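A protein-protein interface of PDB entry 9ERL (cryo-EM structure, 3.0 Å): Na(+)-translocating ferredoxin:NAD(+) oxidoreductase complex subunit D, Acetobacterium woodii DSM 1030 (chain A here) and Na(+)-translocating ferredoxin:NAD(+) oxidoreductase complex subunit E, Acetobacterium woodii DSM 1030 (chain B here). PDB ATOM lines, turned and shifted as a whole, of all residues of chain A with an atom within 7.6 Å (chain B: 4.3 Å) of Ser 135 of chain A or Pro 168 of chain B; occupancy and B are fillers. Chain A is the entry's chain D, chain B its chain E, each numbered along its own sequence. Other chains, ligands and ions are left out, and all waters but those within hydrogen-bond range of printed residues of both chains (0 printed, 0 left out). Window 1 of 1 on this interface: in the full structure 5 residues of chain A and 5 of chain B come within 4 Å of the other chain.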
ATOM      1  N   VAL A 101     -11.574  12.634  -8.767  1.00  0.00           N
ATOM      2  CA  VAL A 101     -11.538  11.177  -8.889  1.00  0.00           C
ATOM      3  C   VAL A 101     -11.671  10.756 -10.348  1.00  0.00           C
ATOM      4  O   VAL A 101     -10.949   9.868 -10.824  1.00  0.00           O
ATOM      5  CB  VAL A 101     -12.633  10.545  -8.009  1.00  0.00           C
ATOM      6  CG1 VAL A 101     -12.780   9.066  -8.313  1.00  0.00           C
ATOM      7  CG2 VAL A 101     -12.311  10.749  -6.541  1.00  0.00           C
ATOM      8  N   ALA A 128     -14.311   7.051 -17.821  1.00  0.00           N
ATOM      9  CA  ALA A 128     -14.385   7.683 -16.508  1.00  0.00           C
ATOM     10  C   ALA A 128     -15.815   8.069 -16.148  1.00  0.00           C
ATOM     11  O   ALA A 128     -16.220   7.927 -14.989  1.00  0.00           O
ATOM     12  CB  ALA A 128     -13.478   8.910 -16.463  1.00  0.00           C
ATOM     13  N   ARG A 129     -16.587   8.555 -17.123  1.00  0.00           N
ATOM     14  CA  ARG A 129     -17.988   8.885 -16.873  1.00  0.00           C
ATOM     15  C   ARG A 129     -18.796   7.645 -16.503  1.00  0.00           C
ATOM     16  O   ARG A 129     -19.625   7.687 -15.586  1.00  0.00           O
ATOM     17  CB  ARG A 129     -18.588   9.563 -18.100  1.00  0.00           C
ATOM     18  CG  ARG A 129     -19.916  10.224 -17.835  1.00  0.00           C
ATOM     19  CD  ARG A 129     -20.813  10.225 -19.056  1.00  0.00           C
ATOM     20  NE  ARG A 129     -21.994  11.043 -18.818  1.00  0.00           N
ATOM     21  CZ  ARG A 129     -23.047  10.652 -18.115  1.00  0.00           C
ATOM     22  NH1 ARG A 129     -23.125   9.437 -17.602  1.00  0.00           N
ATOM     23  NH2 ARG A 129     -24.048  11.506 -17.919  1.00  0.00           N
ATOM     24  N   ALA A 130     -18.573   6.536 -17.212  1.00  0.00           N
ATOM     25  CA  ALA A 130     -19.255   5.287 -16.896  1.00  0.00           C
ATOM     26  C   ALA A 130     -18.859   4.739 -15.532  1.00  0.00           C
ATOM     27  O   ALA A 130     -19.704   4.156 -14.845  1.00  0.00           O
ATOM     28  CB  ALA A 130     -18.974   4.244 -17.977  1.00  0.00           C
ATOM     29  N   PHE A 131     -17.594   4.895 -15.136  1.00  0.00           N
ATOM     30  CA  PHE A 131     -17.170   4.504 -13.795  1.00  0.00           C
ATOM     31  C   PHE A 131     -17.824   5.364 -12.716  1.00  0.00           C
ATOM     32  O   PHE A 131     -18.273   4.831 -11.693  1.00  0.00           O
ATOM     33  CB  PHE A 131     -15.641   4.567 -13.712  1.00  0.00           C
ATOM     34  CG  PHE A 131     -15.103   4.909 -12.349  1.00  0.00           C
ATOM     35  CD1 PHE A 131     -15.023   3.946 -11.358  1.00  0.00           C
ATOM     36  CD2 PHE A 131     -14.632   6.183 -12.075  1.00  0.00           C
ATOM     37  CE1 PHE A 131     -14.512   4.254 -10.110  1.00  0.00           C
ATOM     38  CE2 PHE A 131     -14.122   6.496 -10.831  1.00  0.00           C
ATOM     39  CZ  PHE A 131     -14.062   5.531  -9.848  1.00  0.00           C
ATOM     40  N   LEU A 132     -17.900   6.683 -12.933  1.00  0.00           N
ATOM     41  CA  LEU A 132     -18.549   7.564 -11.965  1.00  0.00           C
ATOM     42  C   LEU A 132     -20.039   7.280 -11.838  1.00  0.00           C
ATOM     43  O   LEU A 132     -20.581   7.332 -10.729  1.00  0.00           O
ATOM     44  CB  LEU A 132     -18.338   9.029 -12.347  1.00  0.00           C
ATOM     45  CG  LEU A 132     -16.946   9.634 -12.180  1.00  0.00           C
ATOM     46  CD1 LEU A 132     -16.891  10.994 -12.842  1.00  0.00           C
ATOM     47  CD2 LEU A 132     -16.590   9.740 -10.712  1.00  0.00           C
ATOM     48  N   LEU A 133     -20.720   7.000 -12.952  1.00  0.00           N
ATOM     49  CA  LEU A 133     -22.154   6.732 -12.893  1.00  0.00           C
ATOM     50  C   LEU A 133     -22.449   5.441 -12.137  1.00  0.00           C
ATOM     51  O   LEU A 133     -23.448   5.352 -11.415  1.00  0.00           O
ATOM     52  CB  LEU A 133     -22.736   6.676 -14.306  1.00  0.00           C
ATOM     53  CG  LEU A 133     -24.200   6.253 -14.460  1.00  0.00           C
ATOM     54  CD1 LEU A 133     -25.129   7.275 -13.833  1.00  0.00           C
ATOM     55  CD2 LEU A 133     -24.547   6.042 -15.923  1.00  0.00           C
ATOM     56  N   ALA A 134     -21.594   4.429 -12.291  1.00  0.00           N
ATOM     57  CA  ALA A 134     -21.817   3.162 -11.605  1.00  0.00           C
ATOM     58  C   ALA A 134     -21.443   3.246 -10.130  1.00  0.00           C
ATOM     59  O   ALA A 134     -22.108   2.638  -9.284  1.00  0.00           O
ATOM     60  CB  ALA A 134     -21.031   2.047 -12.293  1.00  0.00           C
ATOM     61  N   SER A 135     -20.375   3.978  -9.799  1.00  0.00           N
ATOM     62  CA  SER A 135     -19.920   4.021  -8.412  1.00  0.00           C
ATOM     63  C   SER A 135     -20.846   4.857  -7.533  1.00  0.00           C
ATOM     64  O   SER A 135     -21.191   4.442  -6.422  1.00  0.00           O
ATOM     65  CB  SER A 135     -18.492   4.555  -8.345  1.00  0.00           C
ATOM     66  OG  SER A 135     -17.653   3.866  -9.252  1.00  0.00           O
ATOM     67  N   TRP A 136     -21.257   6.033  -8.007  1.00  0.00           N
ATOM     68  CA  TRP A 136     -22.073   6.968  -7.228  1.00  0.00           C
ATOM     69  C   TRP A 136     -23.310   7.338  -8.033  1.00  0.00           C
ATOM     70  O   TRP A 136     -23.362   8.406  -8.658  1.00  0.00           O
ATOM     71  CB  TRP A 136     -21.277   8.219  -6.851  1.00  0.00           C
ATOM     72  CG  TRP A 136     -20.182   7.973  -5.855  1.00  0.00           C
ATOM     73  CD1 TRP A 136     -20.322   7.814  -4.508  1.00  0.00           C
ATOM     74  CD2 TRP A 136     -18.780   7.853  -6.128  1.00  0.00           C
ATOM     75  NE1 TRP A 136     -19.097   7.604  -3.926  1.00  0.00           N
ATOM     76  CE2 TRP A 136     -18.134   7.624  -4.900  1.00  0.00           C
ATOM     77  CE3 TRP A 136     -18.011   7.919  -7.293  1.00  0.00           C
ATOM     78  CZ2 TRP A 136     -16.757   7.457  -4.803  1.00  0.00           C
ATOM     79  CZ3 TRP A 136     -16.645   7.754  -7.194  1.00  0.00           C
ATOM     80  CH2 TRP A 136     -16.032   7.527  -5.959  1.00  0.00           C
ATOM     81  N   PRO A 137     -24.332   6.478  -8.041  1.00  0.00           N
ATOM     82  CA  PRO A 137     -25.535   6.791  -8.827  1.00  0.00           C
ATOM     83  C   PRO A 137     -26.402   7.871  -8.206  1.00  0.00           C
ATOM     84  O   PRO A 137     -27.234   8.455  -8.908  1.00  0.00           O
ATOM     85  CB  PRO A 137     -26.267   5.446  -8.891  1.00  0.00           C
ATOM     86  CG  PRO A 137     -25.845   4.741  -7.655  1.00  0.00           C
ATOM     87  CD  PRO A 137     -24.433   5.170  -7.370  1.00  0.00           C
ATOM     88  N   GLY A 138     -26.252   8.140  -6.907  1.00  0.00           N
ATOM     89  CA  GLY A 138     -27.050   9.175  -6.274  1.00  0.00           C
ATOM     90  C   GLY A 138     -26.717  10.575  -6.746  1.00  0.00           C
ATOM     91  O   GLY A 138     -27.606  11.424  -6.853  1.00  0.00           O
ATOM     92  N   HIS A 139     -25.442  10.840  -7.026  1.00  0.00           N
ATOM     93  CA  HIS A 139     -24.992  12.175  -7.402  1.00  0.00           C
ATOM     94  C   HIS A 139     -25.087  12.448  -8.896  1.00  0.00           C
ATOM     95  O   HIS A 139     -24.756  13.558  -9.322  1.00  0.00           O
ATOM     96  CB  HIS A 139     -23.543  12.387  -6.952  1.00  0.00           C
ATOM     97  CG  HIS A 139     -23.385  12.584  -5.477  1.00  0.00           C
ATOM     98  ND1 HIS A 139     -24.121  13.506  -4.765  1.00  0.00           N
ATOM     99  CD2 HIS A 139     -22.571  11.979  -4.580  1.00  0.00           C
ATOM    100  CE1 HIS A 139     -23.769  13.460  -3.493  1.00  0.00           C
ATOM    101  NE2 HIS A 139     -22.831  12.541  -3.354  1.00  0.00           N
ATOM    102  N   MET A 140     -25.523  11.476  -9.700  1.00  0.00           N
ATOM    103  CA  MET A 140     -25.498  11.618 -11.150  1.00  0.00           C
ATOM    104  C   MET A 140     -26.799  11.263 -11.856  1.00  0.00           C
ATOM    105  O   MET A 140     -26.766  11.053 -13.073  1.00  0.00           O
ATOM    106  CB  MET A 140     -24.379  10.751 -11.754  1.00  0.00           C
ATOM    107  CG  MET A 140     -22.975  11.072 -11.262  1.00  0.00           C
ATOM    108  SD  MET A 140     -22.085  12.201 -12.350  1.00  0.00           S
ATOM    109  CE  MET A 140     -21.750  11.140 -13.750  1.00  0.00           C
ATOM    110  N   GLY B 152     -14.775  -1.054  -1.116  1.00  0.00           N
ATOM    111  CA  GLY B 152     -16.151  -1.112  -1.566  1.00  0.00           C
ATOM    112  C   GLY B 152     -17.216  -1.145  -0.496  1.00  0.00           C
ATOM    113  O   GLY B 152     -18.401  -1.054  -0.822  1.00  0.00           O
ATOM    114  N   ALA B 153     -16.840  -1.289   0.775  1.00  0.00           N
ATOM    115  CA  ALA B 153     -17.807  -1.289   1.865  1.00  0.00           C
ATOM    116  C   ALA B 153     -17.404  -0.433   3.055  1.00  0.00           C
ATOM    117  O   ALA B 153     -18.271  -0.122   3.879  1.00  0.00           O
ATOM    118  CB  ALA B 153     -18.066  -2.721   2.354  1.00  0.00           C
ATOM    119  N   TYR B 166     -19.877   7.403   5.289  1.00  0.00           N
ATOM    120  CA  TYR B 166     -19.029   7.065   4.155  1.00  0.00           C
ATOM    121  C   TYR B 166     -19.870   6.600   2.973  1.00  0.00           C
ATOM    122  O   TYR B 166     -20.828   5.837   3.131  1.00  0.00           O
ATOM    123  CB  TYR B 166     -18.033   5.979   4.563  1.00  0.00           C
ATOM    124  CG  TYR B 166     -17.079   5.539   3.477  1.00  0.00           C
ATOM    125  CD1 TYR B 166     -16.174   6.427   2.915  1.00  0.00           C
ATOM    126  CD2 TYR B 166     -17.076   4.228   3.023  1.00  0.00           C
ATOM    127  CE1 TYR B 166     -15.298   6.023   1.926  1.00  0.00           C
ATOM    128  CE2 TYR B 166     -16.206   3.815   2.036  1.00  0.00           C
ATOM    129  CZ  TYR B 166     -15.321   4.715   1.490  1.00  0.00           C
ATOM    130  OH  TYR B 166     -14.453   4.305   0.506  1.00  0.00           O
ATOM    131  N   GLU B 167     -19.512   7.071   1.781  1.00  0.00           N
ATOM    132  CA  GLU B 167     -20.167   6.651   0.548  1.00  0.00           C
ATOM    133  C   GLU B 167     -19.244   5.708  -0.206  1.00  0.00           C
ATOM    134  O   GLU B 167     -18.226   6.156  -0.756  1.00  0.00           O
ATOM    135  CB  GLU B 167     -20.521   7.858  -0.319  1.00  0.00           C
ATOM    136  CG  GLU B 167     -21.071   9.035   0.463  1.00  0.00           C
ATOM    137  CD  GLU B 167     -21.890   9.972  -0.397  1.00  0.00           C
ATOM    138  OE1 GLU B 167     -22.682   9.478  -1.224  1.00  0.00           O
ATOM    139  OE2 GLU B 167     -21.740  11.201  -0.247  1.00  0.00           O
ATOM    140  N   PRO B 168     -19.548   4.414  -0.264  1.00  0.00           N
ATOM    141  CA  PRO B 168     -18.595   3.451  -0.820  1.00  0.00           C
ATOM    142  C   PRO B 168     -18.484   3.548  -2.333  1.00  0.00           C
ATOM    143  O   PRO B 168     -19.354   4.083  -3.024  1.00  0.00           O
ATOM    144  CB  PRO B 168     -19.175   2.095  -0.400  1.00  0.00           C
ATOM    145  CG  PRO B 168     -20.210   2.407   0.645  1.00  0.00           C
ATOM    146  CD  PRO B 168     -20.738   3.748   0.283  1.00  0.00           C
ATOM    147  N   VAL B 169     -17.377   3.012  -2.844  1.00  0.00           N
ATOM    148  CA  VAL B 169     -17.181   2.827  -4.281  1.00  0.00           C
ATOM    149  C   VAL B 169     -17.839   1.501  -4.644  1.00  0.00           C
ATOM    150  O   VAL B 169     -17.279   0.432  -4.397  1.00  0.00           O
ATOM    151  CB  VAL B 169     -15.699   2.847  -4.662  1.00  0.00           C
ATOM    152  CG1 VAL B 169     -15.540   2.993  -6.163  1.00  0.00           C
ATOM    153  CG2 VAL B 169     -14.977   3.965  -3.934  1.00  0.00           C
ATOM    154  N   LEU B 170     -19.029   1.559  -5.236  1.00  0.00           N
ATOM    155  CA  LEU B 170     -19.806   0.357  -5.503  1.00  0.00           C
ATOM    156  C   LEU B 170     -19.306  -0.427  -6.708  1.00  0.00           C
ATOM    157  O   LEU B 170     -19.814  -1.522  -6.962  1.00  0.00           O
ATOM    158  CB  LEU B 170     -21.283   0.710  -5.699  1.00  0.00           C
ATOM    159  CG  LEU B 170     -22.017   1.310  -4.500  1.00  0.00           C
ATOM    160  CD1 LEU B 170     -23.403   1.775  -4.910  1.00  0.00           C
ATOM    161  CD2 LEU B 170     -22.100   0.313  -3.360  1.00  0.00           C
ATOM    162  N   LEU B 171     -18.338   0.096  -7.457  1.00  0.00           N
ATOM    163  CA  LEU B 171     -17.760  -0.655  -8.562  1.00  0.00           C
ATOM    164  C   LEU B 171     -16.782  -1.724  -8.098  1.00  0.00           C
ATOM    165  O   LEU B 171     -16.578  -2.711  -8.814  1.00  0.00           O
ATOM    166  CB  LEU B 171     -17.059   0.291  -9.542  1.00  0.00           C
ATOM    167  CG  LEU B 171     -16.770  -0.268 -10.938  1.00  0.00           C
ATOM    168  CD1 LEU B 171     -17.933  -0.015 -11.877  1.00  0.00           C
ATOM    169  CD2 LEU B 171     -15.488   0.318 -11.503  1.00  0.00           C
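The backbone carbonyl oxygen (O) of Phe 131 of chain A lies within hydrogen-bond range of the side-chain hydroxyl (OG) of Ser 135 of chain A (2.7 Å).
Among the printed residues, merely in contact across the chains: His 139 of chain A with Glu 167 of chain B, Trp 136 of chain A with Glu 167 of chain B, Ser 135 of chain A with Leu 171 of chain B, Trp 136 of chain A with Pro 168 of chain B, Phe 131 of chain A with Leu 171 of chain B, Ala 134 of chain A with Leu 171 of chain B, Ser 135 of chain A with Leu 170 of chain B, Ser 135 of chain A with Val 169 of chain B and Ser 135 of chain A with Pro 168 of chain B.
Of the 8 printed residues of chain B, 5 touch a printed residue of chain A. Hydrophobic or aromatic side chains of chain B within 4 Å of the printed part of chain A: Val 169, Leu 170 and Leu 171. Along chain B the printed residues that touch a printed residue of chain A span positions 167 to 171. Of the 14 printed residues of chain A, 5 touch a printed residue of chain B. Hydrophobic or aromatic side chains of chain A within 4 Å of the printed part of chain B: Phe 131, Ala 134, Trp 136 and His 139. Along chain A the printed residues that touch a printed residue of chain B span positions 131 to 139. Among the printed residues, 9 pairs touch across the chains.
Printed residues of chain B within 4 Å of Phe 131 of chain A: Leu 171. Ser 135 of chain A touches just these residues of chain B: Pro 168 (3.9 Å), Val 169 (3.8 Å), Leu 170 (3.8 Å) and Leu 171 (3.6 Å). Of the printed residues of chain A, Glu 167 of chain B touches Trp 136 (3.6 Å) and His 139 (3.6 Å). Pro 168 of chain B touches two residues of chain A. The nearest printed residue of chain B that does not touch Trp 136 of chain A is Val 169 of chain B (4.01 Å).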
